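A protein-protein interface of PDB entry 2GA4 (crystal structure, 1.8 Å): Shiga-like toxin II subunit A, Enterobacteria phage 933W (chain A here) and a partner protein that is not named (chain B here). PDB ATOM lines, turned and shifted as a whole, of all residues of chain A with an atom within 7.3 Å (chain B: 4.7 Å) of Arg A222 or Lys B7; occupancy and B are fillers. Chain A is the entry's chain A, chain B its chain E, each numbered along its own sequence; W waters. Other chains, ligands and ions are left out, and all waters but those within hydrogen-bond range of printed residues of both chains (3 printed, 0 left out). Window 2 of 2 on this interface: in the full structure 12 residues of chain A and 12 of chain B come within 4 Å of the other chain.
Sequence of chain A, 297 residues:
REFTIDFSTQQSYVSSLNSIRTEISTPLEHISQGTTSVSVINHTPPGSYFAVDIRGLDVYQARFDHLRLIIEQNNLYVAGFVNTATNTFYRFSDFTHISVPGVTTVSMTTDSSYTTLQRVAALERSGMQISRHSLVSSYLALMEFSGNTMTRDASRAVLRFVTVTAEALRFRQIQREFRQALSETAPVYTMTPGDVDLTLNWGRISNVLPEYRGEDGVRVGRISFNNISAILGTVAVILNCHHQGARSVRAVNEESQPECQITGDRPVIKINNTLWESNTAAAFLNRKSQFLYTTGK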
ATOM      1  N   PRO A 193      22.524  10.746  -4.496  1.00  0.00           N
ATOM      2  CA  PRO A 193      21.450   9.767  -4.599  1.00  0.00           C
ATOM      3  C   PRO A 193      21.953   8.693  -5.532  1.00  0.00           C
ATOM      4  O   PRO A 193      21.688   7.513  -5.306  1.00  0.00           O
ATOM      5  CB  PRO A 193      20.304  10.580  -5.199  1.00  0.00           C
ATOM      6  CG  PRO A 193      20.539  11.935  -4.549  1.00  0.00           C
ATOM      7  CD  PRO A 193      22.017  12.121  -4.681  1.00  0.00           C
ATOM      8  N   GLY A 194      22.708   9.090  -6.560  1.00  0.00           N
ATOM      9  CA  GLY A 194      23.228   8.112  -7.516  1.00  0.00           C
ATOM     10  C   GLY A 194      24.208   7.168  -6.838  1.00  0.00           C
ATOM     11  O   GLY A 194      24.225   5.968  -7.117  1.00  0.00           O
ATOM     12  N   ASP A 197      22.144   4.875  -4.828  1.00  0.00           N
ATOM     13  CA  ASP A 197      21.496   3.887  -5.663  1.00  0.00           C
ATOM     14  C   ASP A 197      22.459   2.804  -6.089  1.00  0.00           C
ATOM     15  O   ASP A 197      22.106   1.624  -6.113  1.00  0.00           O
ATOM     16  CB  ASP A 197      20.884   4.525  -6.905  1.00  0.00           C
ATOM     17  CG  ASP A 197      19.386   4.711  -6.755  1.00  0.00           C
ATOM     18  OD1 ASP A 197      18.799   4.065  -5.852  1.00  0.00           O
ATOM     19  OD2 ASP A 197      18.795   5.478  -7.540  1.00  0.00           O
ATOM     20  N   LEU A 200      22.920   0.273  -3.416  1.00  0.00           N
ATOM     21  CA  LEU A 200      21.735  -0.528  -3.167  1.00  0.00           C
ATOM     22  C   LEU A 200      21.513  -1.569  -4.267  1.00  0.00           C
ATOM     23  O   LEU A 200      20.642  -2.443  -4.158  1.00  0.00           O
ATOM     24  CB  LEU A 200      20.528   0.399  -3.086  1.00  0.00           C
ATOM     25  CG  LEU A 200      20.595   1.411  -1.929  1.00  0.00           C
ATOM     26  CD1 LEU A 200      19.486   2.464  -2.084  1.00  0.00           C
ATOM     27  CD2 LEU A 200      20.516   0.674  -0.635  1.00  0.00           C
ATOM     28  N   ASN A 201      22.276  -1.473  -5.338  1.00  0.00           N
ATOM     29  CA  ASN A 201      22.077  -2.399  -6.450  1.00  0.00           C
ATOM     30  C   ASN A 201      23.287  -3.262  -6.711  1.00  0.00           C
ATOM     31  O   ASN A 201      23.407  -3.839  -7.774  1.00  0.00           O
ATOM     32  CB  ASN A 201      21.799  -1.604  -7.710  1.00  0.00           C
ATOM     33  CG  ASN A 201      20.387  -1.112  -7.768  1.00  0.00           C
ATOM     34  OD1 ASN A 201      19.542  -1.779  -8.344  1.00  0.00           O
ATOM     35  ND2 ASN A 201      20.114   0.041  -7.154  1.00  0.00           N
ATOM     36  N   ARG A 204      22.479  -6.860  -7.620  1.00  0.00           N
ATOM     37  CA  ARG A 204      21.833  -6.983  -8.915  1.00  0.00           C
ATOM     38  C   ARG A 204      22.835  -6.748 -10.030  1.00  0.00           C
ATOM     39  O   ARG A 204      22.824  -7.435 -11.068  1.00  0.00           O
ATOM     40  CB  ARG A 204      20.678  -5.982  -9.000  1.00  0.00           C
ATOM     41  CG  ARG A 204      19.645  -6.358  -7.956  1.00  0.00           C
ATOM     42  CD  ARG A 204      18.636  -5.241  -7.798  1.00  0.00           C
ATOM     43  NE  ARG A 204      17.788  -5.130  -8.994  1.00  0.00           N
ATOM     44  CZ  ARG A 204      16.879  -4.172  -9.142  1.00  0.00           C
ATOM     45  NH1 ARG A 204      16.714  -3.246  -8.156  1.00  0.00           N
ATOM     46  NH2 ARG A 204      16.127  -4.135 -10.226  1.00  0.00           N
ATOM     47  N   ARG A 219      21.318  -2.244 -18.261  1.00  0.00           N
ATOM     48  CA  ARG A 219      20.281  -1.625 -17.460  1.00  0.00           C
ATOM     49  C   ARG A 219      19.980  -2.547 -16.329  1.00  0.00           C
ATOM     50  O   ARG A 219      19.634  -3.688 -16.541  1.00  0.00           O
ATOM     51  CB  ARG A 219      19.029  -1.372 -18.335  1.00  0.00           C
ATOM     52  CG  ARG A 219      19.294  -0.318 -19.426  1.00  0.00           C
ATOM     53  CD  ARG A 219      19.324   1.099 -18.822  1.00  0.00           C
ATOM     54  NE  ARG A 219      17.970   1.536 -18.439  1.00  0.00           N
ATOM     55  CZ  ARG A 219      17.490   1.550 -17.202  1.00  0.00           C
ATOM     56  NH1 ARG A 219      18.238   1.181 -16.154  1.00  0.00           N
ATOM     57  NH2 ARG A 219      16.212   1.902 -17.002  1.00  0.00           N
ATOM     58  N   VAL A 220      20.169  -2.057 -15.112  1.00  0.00           N
ATOM     59  CA  VAL A 220      19.888  -2.881 -13.961  1.00  0.00           C
ATOM     60  C   VAL A 220      19.069  -2.013 -13.059  1.00  0.00           C
ATOM     61  O   VAL A 220      19.589  -1.135 -12.375  1.00  0.00           O
ATOM     62  CB  VAL A 220      21.197  -3.311 -13.254  1.00  0.00           C
ATOM     63  CG1 VAL A 220      20.843  -4.142 -12.020  1.00  0.00           C
ATOM     64  CG2 VAL A 220      22.016  -4.197 -14.217  1.00  0.00           C
ATOM     65  N   GLY A 221      17.758  -2.239 -13.072  1.00  0.00           N
ATOM     66  CA  GLY A 221      16.896  -1.407 -12.251  1.00  0.00           C
ATOM     67  C   GLY A 221      17.068   0.055 -12.629  1.00  0.00           C
ATOM     68  O   GLY A 221      16.947   0.439 -13.786  1.00  0.00           O
ATOM     69  N   ARG A 222      17.365   0.868 -11.633  1.00  0.00           N
ATOM     70  CA  ARG A 222      17.557   2.302 -11.825  1.00  0.00           C
ATOM     71  C   ARG A 222      18.939   2.632 -12.371  1.00  0.00           C
ATOM     72  O   ARG A 222      19.213   3.795 -12.676  1.00  0.00           O
ATOM     73  CB  ARG A 222      17.392   2.990 -10.479  1.00  0.00           C
ATOM     74  CG  ARG A 222      15.965   2.762  -9.856  1.00  0.00           C
ATOM     75  CD  ARG A 222      15.914   3.056  -8.366  1.00  0.00           C
ATOM     76  NE  ARG A 222      16.329   4.410  -7.991  1.00  0.00           N
ATOM     77  CZ  ARG A 222      15.529   5.465  -7.984  1.00  0.00           C
ATOM     78  NH1 ARG A 222      14.245   5.364  -8.370  1.00  0.00           N
ATOM     79  NH2 ARG A 222      15.962   6.615  -7.458  1.00  0.00           N
ATOM     80  N   ILE A 223      19.765   1.608 -12.530  1.00  0.00           N
ATOM     81  CA  ILE A 223      21.148   1.806 -12.955  1.00  0.00           C
ATOM     82  C   ILE A 223      21.307   1.640 -14.436  1.00  0.00           C
ATOM     83  O   ILE A 223      20.778   0.698 -15.042  1.00  0.00           O
ATOM     84  CB  ILE A 223      22.118   0.804 -12.244  1.00  0.00           C
ATOM     85  CG1 ILE A 223      21.937   0.833 -10.708  1.00  0.00           C
ATOM     86  CG2 ILE A 223      23.592   1.143 -12.630  1.00  0.00           C
ATOM     87  CD1 ILE A 223      22.058   2.253 -10.089  1.00  0.00           C
ATOM     88  N   SER A 224      22.032   2.572 -15.059  1.00  0.00           N
ATOM     89  CA  SER A 224      22.235   2.484 -16.496  1.00  0.00           C
ATOM     90  C   SER A 224      23.701   2.726 -16.810  1.00  0.00           C
ATOM     91  O   SER A 224      24.302   3.667 -16.264  1.00  0.00           O
ATOM     92  CB  SER A 224      21.421   3.571 -17.234  1.00  0.00           C
ATOM     93  OG  SER A 224      20.041   3.463 -16.924  1.00  0.00           O
ATOM     94  N   GLU A 277      18.722  -6.404 -16.815  1.00  0.00           N
ATOM     95  CA  GLU A 277      18.517  -7.355 -15.740  1.00  0.00           C
ATOM     96  C   GLU A 277      17.113  -7.893 -16.089  1.00  0.00           C
ATOM     97  O   GLU A 277      16.164  -7.116 -16.221  1.00  0.00           O
ATOM     98  CB  GLU A 277      18.426  -6.614 -14.404  1.00  0.00           C
ATOM     99  CG  GLU A 277      18.058  -7.606 -13.290  1.00  0.00           C
ATOM    100  CD  GLU A 277      17.666  -6.861 -12.088  1.00  0.00           C
ATOM    101  OE1 GLU A 277      16.656  -6.138 -12.151  1.00  0.00           O
ATOM    102  OE2 GLU A 277      18.374  -6.991 -11.089  1.00  0.00           O
ATOM    103  N   THR A 280      14.174  -6.587 -14.063  1.00  0.00           N
ATOM    104  CA  THR A 280      13.734  -5.219 -14.279  1.00  0.00           C
ATOM    105  C   THR A 280      12.740  -5.193 -15.409  1.00  0.00           C
ATOM    106  O   THR A 280      11.698  -4.551 -15.318  1.00  0.00           O
ATOM    107  CB  THR A 280      14.902  -4.316 -14.660  1.00  0.00           C
ATOM    108  OG1 THR A 280      15.799  -4.236 -13.548  1.00  0.00           O
ATOM    109  CG2 THR A 280      14.383  -2.921 -14.992  1.00  0.00           C
ATOM    110  N   GLY B   6      13.162  14.618 -11.155  1.00  0.00           N
ATOM    111  CA  GLY B   6      14.161  13.759 -10.563  1.00  0.00           C
ATOM    112  C   GLY B   6      13.689  12.330 -10.604  1.00  0.00           C
ATOM    113  O   GLY B   6      12.638  12.057 -11.132  1.00  0.00           O
ATOM    114  N   LYS B   7      14.479  11.416 -10.076  1.00  0.00           N
ATOM    115  CA  LYS B   7      14.043  10.040 -10.068  1.00  0.00           C
ATOM    116  C   LYS B   7      13.082   9.948  -8.913  1.00  0.00           C
ATOM    117  O   LYS B   7      13.038  10.824  -8.027  1.00  0.00           O
ATOM    118  CB  LYS B   7      15.198   9.077  -9.852  1.00  0.00           C
ATOM    119  CG  LYS B   7      16.199   9.097 -10.989  1.00  0.00           C
ATOM    120  CD  LYS B   7      17.260   8.004 -10.798  1.00  0.00           C
ATOM    121  CE  LYS B   7      18.296   8.040 -11.924  1.00  0.00           C
ATOM    122  NZ  LYS B   7      19.048   6.744 -11.883  1.00  0.00           N
ATOM    123  N   ILE B   8      12.312   8.875  -8.902  1.00  0.00           N
ATOM    124  CA  ILE B   8      11.370   8.692  -7.825  1.00  0.00           C
ATOM    125  C   ILE B   8      12.061   8.039  -6.651  1.00  0.00           C
ATOM    126  O   ILE B   8      12.598   6.947  -6.774  1.00  0.00           O
ATOM    127  CB  ILE B   8      10.171   7.839  -8.300  1.00  0.00           C
ATOM    128  CG1 ILE B   8       9.407   8.633  -9.362  1.00  0.00           C
ATOM    129  CG2 ILE B   8       9.280   7.485  -7.106  1.00  0.00           C
ATOM    130  CD1 ILE B   8       8.403   7.776 -10.086  1.00  0.00           C
ATOM    131  N   GLU B   9      12.033   8.729  -5.521  1.00  0.00           N
ATOM    132  CA  GLU B   9      12.676   8.260  -4.293  1.00  0.00           C
ATOM    133  C   GLU B   9      11.876   7.143  -3.645  1.00  0.00           C
ATOM    134  O   GLU B   9      12.458   6.200  -3.153  1.00  0.00           O
ATOM    135  CB  GLU B   9      12.880   9.414  -3.324  1.00  0.00           C
ATOM    136  CG  GLU B   9      13.616   8.936  -2.112  1.00  0.00           C
ATOM    137  CD  GLU B   9      13.940  10.046  -1.154  1.00  0.00           C
ATOM    138  OE1 GLU B   9      13.910  11.214  -1.596  1.00  0.00           O
ATOM    139  OE2 GLU B   9      14.227   9.728   0.030  1.00  0.00           O
ATOM    140  N   LYS B  22       7.725  10.553  -4.182  1.00  0.00           N
ATOM    141  CA  LYS B  22       8.632  11.590  -3.695  1.00  0.00           C
ATOM    142  C   LYS B  22       9.627  11.824  -4.797  1.00  0.00           C
ATOM    143  O   LYS B  22      10.268  10.892  -5.277  1.00  0.00           O
ATOM    144  CB  LYS B  22       9.359  11.128  -2.456  1.00  0.00           C
ATOM    145  CG  LYS B  22      10.234  12.223  -1.915  1.00  0.00           C
ATOM    146  CD  LYS B  22      10.481  11.978  -0.457  1.00  0.00           C
ATOM    147  CE  LYS B  22      11.588  12.897   0.080  1.00  0.00           C
ATOM    148  NZ  LYS B  22      11.685  12.726   1.556  1.00  0.00           N
ATOM    149  N   VAL B  23       9.725  13.069  -5.237  1.00  0.00           N
ATOM    150  CA  VAL B  23      10.630  13.439  -6.304  1.00  0.00           C
ATOM    151  C   VAL B  23      11.352  14.728  -5.865  1.00  0.00           C
ATOM    152  O   VAL B  23      10.707  15.687  -5.456  1.00  0.00           O
ATOM    153  CB  VAL B  23       9.857  13.748  -7.567  1.00  0.00           C
ATOM    154  CG1 VAL B  23      10.830  14.057  -8.715  1.00  0.00           C
ATOM    155  CG2 VAL B  23       8.965  12.489  -7.956  1.00  0.00           C
ATOM    156  N   ASP B  24      12.670  14.720  -5.959  1.00  0.00           N
ATOM    157  CA  ASP B  24      13.477  15.899  -5.600  1.00  0.00           C
ATOM    158  C   ASP B  24      13.106  16.401  -4.202  1.00  0.00           C
ATOM    159  O   ASP B  24      12.879  17.586  -3.988  1.00  0.00           O
ATOM    160  CB  ASP B  24      13.266  17.006  -6.629  1.00  0.00           C
ATOM    161  CG  ASP B  24      14.330  18.091  -6.531  1.00  0.00           C
ATOM    162  OD1 ASP B  24      15.492  17.732  -6.247  1.00  0.00           O
ATOM    163  OD2 ASP B  24      13.984  19.275  -6.738  1.00  0.00           O
ATOM    164  N   GLN B  43       9.929   4.505 -11.356  1.00  0.00           N
ATOM    165  CA  GLN B  43      10.724   4.391 -10.167  1.00  0.00           C
ATOM    166  C   GLN B  43      11.718   3.237 -10.265  1.00  0.00           C
ATOM    167  O   GLN B  43      12.899   3.421 -10.002  1.00  0.00           O
ATOM    168  CB  GLN B  43       9.823   4.165  -8.918  1.00  0.00           C
ATOM    169  CG  GLN B  43      10.633   3.894  -7.654  1.00  0.00           C
ATOM    170  CD  GLN B  43       9.720   3.590  -6.476  1.00  0.00           C
ATOM    171  OE1 GLN B  43       8.487   3.614  -6.627  1.00  0.00           O
ATOM    172  NE2 GLN B  43      10.300   3.301  -5.314  1.00  0.00           N
ATOM    173  N   LEU B  44      11.252   2.055 -10.680  1.00  0.00           N
ATOM    174  CA  LEU B  44      12.153   0.920 -10.659  1.00  0.00           C
ATOM    175  C   LEU B  44      13.185   0.902 -11.778  1.00  0.00           C
ATOM    176  O   LEU B  44      14.184   0.208 -11.672  1.00  0.00           O
ATOM    177  CB  LEU B  44      11.341  -0.376 -10.634  1.00  0.00           C
ATOM    178  CG  LEU B  44      10.564  -0.724 -11.888  1.00  0.00           C
ATOM    179  CD1 LEU B  44      11.394  -1.651 -12.781  1.00  0.00           C
ATOM    180  CD2 LEU B  44       9.250  -1.473 -11.450  1.00  0.00           C
ATOM    181  N   THR B  45      12.946   1.698 -12.811  1.00  0.00           N
ATOM    182  CA  THR B  45      13.866   1.795 -13.948  1.00  0.00           C
ATOM    183  C   THR B  45      14.698   3.070 -13.885  1.00  0.00           C
ATOM    184  O   THR B  45      15.519   3.320 -14.772  1.00  0.00           O
ATOM    185  CB  THR B  45      13.145   1.819 -15.304  1.00  0.00           C
ATOM    186  OG1 THR B  45      12.237   2.938 -15.346  1.00  0.00           O
ATOM    187  CG2 THR B  45      12.392   0.488 -15.537  1.00  0.00           C
ATOM    188  N   GLY B  46      14.461   3.872 -12.851  1.00  0.00           N
ATOM    189  CA  GLY B  46      15.257   5.084 -12.667  1.00  0.00           C
ATOM    190  C   GLY B  46      15.019   6.186 -13.682  1.00  0.00           C
ATOM    191  O   GLY B  46      15.910   6.980 -13.972  1.00  0.00           O
ATOM    192  N   MET B  47      13.817   6.261 -14.216  1.00  0.00           N
ATOM    193  CA  MET B  47      13.505   7.323 -15.151  1.00  0.00           C
ATOM    194  C   MET B  47      13.475   8.641 -14.418  1.00  0.00           C
ATOM    195  O   MET B  47      13.239   8.704 -13.226  1.00  0.00           O
ATOM    196  CB  MET B  47      12.123   7.126 -15.782  1.00  0.00           C
ATOM    197  CG  MET B  47      12.010   5.859 -16.642  1.00  0.00           C
ATOM    198  SD  MET B  47      10.385   5.905 -17.418  1.00  0.00           S
ATOM    199  CE  MET B  47      10.761   6.483 -19.055  1.00  0.00           C
ATOM    200  N   THR B  48      13.745   9.707 -15.148  1.00  0.00           N
ATOM    201  CA  THR B  48      13.612  11.012 -14.562  1.00  0.00           C
ATOM    202  C   THR B  48      12.167  11.440 -14.818  1.00  0.00           C
ATOM    203  O   THR B  48      11.691  11.452 -15.963  1.00  0.00           O
ATOM    204  CB  THR B  48      14.579  12.029 -15.220  1.00  0.00           C
ATOM    205  OG1 THR B  48      15.898  11.615 -14.906  1.00  0.00           O
ATOM    206  CG2 THR B  48      14.324  13.462 -14.688  1.00  0.00           C
HETATM  207  O   HOH W   1      15.275   9.145  -6.147  1.00  0.00           O
HETATM  208  O   HOH W   2      14.591  -1.692  -9.790  1.00  0.00           O
HETATM  209  O   HOH W   3      20.276   6.017  -9.569  1.00  0.00           O
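The backbone carbonyl oxygen (O) of Thr B45 sits at hydrogen-bond distance from the guanidinium group (NH2) of Arg A219. O of Leu B44 sits at hydrogen-bond distance from N of Arg A222. The backbone carbonyl oxygen (O) of Gly A221 sits close to the backbone carbonyl oxygen (O) of Leu B44 (3.5 Å). The guanidinium group of Arg A222 is in hydrogen-bond range of the backbone carbonyl oxygen of Ile B8 (2.8 Å). The guanidinium group (NH1) of Arg A222 lies within hydrogen-bond range of the backbone carbonyl oxygen (O) of Gln B43 (2.9 Å). The backbone carbonyl oxygen (O) of Arg A222 is in hydrogen-bond range of the side-chain amino group (NZ) of Lys B7, 3.1 Å away. O of Thr B45 sits close to O of Gly A221, at 3.4 Å.
Water W3 bridges OD2 of Asp A197 (2.6 Å) and NZ of Lys B7 (2.7 Å). Water W2 bridges O of Leu B44 (2.7 Å) and NH2 of Arg A204 (2.9 Å). Water W1 lies within hydrogen-bond range of the guanidinium group of Arg A222, the backbone NH of Glu B9 and the backbone carbonyl oxygen of Lys B7.
The guanidinium group (NE) of Arg A222 lies within salt-bridge range of the side-chain carboxylate (OD2) of Asp A197. OE1 of Glu A277 lies within hydrogen-bond range of OG1 of Thr A280 (2.5 Å). The guanidinium group (NH2) of Arg A204 lies within hydrogen-bond range of the side-chain hydroxyl (OG1) of Thr A280 (3.3 Å). The backbone NH (N) of Glu A277 lies within hydrogen-bond range of the backbone carbonyl oxygen (O) of Arg A219, 2.9 Å away. The side-chain hydroxyl (OG1) of Thr A280 lies within hydrogen-bond range of the backbone NH (N) of Gly A221 (2.8 Å). NH1 of Arg A219 sits at hydrogen-bond distance from O of Ile A223 (2.8 Å).
Arg A222 touches Thr B45 (CA to C, 3.6 Å). Arg A222 touches Gly B46. Thr A280 touches Leu B44 (O to CD1, 3.9 Å). CG2 of Thr A280 touches CG2 of Thr B45, at 3.99 Å.
Of chain B, only Lys B7 (3.1 Å), Ile B8 (2.8 Å), Gln B43 (2.9 Å), Leu B44 (3.2 Å), Thr B45 (3.6 Å) and Gly B46 (3.5 Å) come within 4 Å of Arg A222. Of chain A, only Arg A222 (3.1 Å) comes within 4 Å of Lys B7. Printed residues of chain B within 4 Å of Thr A280: Leu B44 and Thr B45. Of the printed residues of chain A, Leu B44 touches Gly A221 (3.0 Å), Arg A222 (3.2 Å) and Thr A280 (3.9 Å). Of the printed residues of chain A, Ile B8 touches Arg A222 (2.8 Å). The nearest residue of chain A that does not touch Lys B7 is Asp A197 (4.4 Å). The nearest printed residue of chain A that does not touch Ile B8 is Asp A197 (6.4 Å).
Of the 14 printed residues of chain A, 4 touch a printed residue of chain B. Printed residues of chain A that touch a printed residue of chain B: Arg A219, Gly A221, Arg A222 and Thr A280. Along chain A the printed residues that touch a printed residue of chain B span positions 219 to 280. Of the 13 printed residues of chain B, 6 touch a printed residue of chain A. Printed residues of chain B that touch a printed residue of chain A: Lys B7, Ile B8, Gln B43, Leu B44, Thr B45 and Gly B46. Along chain B the printed residues that touch a printed residue of chain A span positions 7 to 46. Among the printed residues, no Asp or Glu carboxylate lies within 4 Å of a Lys or Arg side-chain nitrogen of the other chain.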
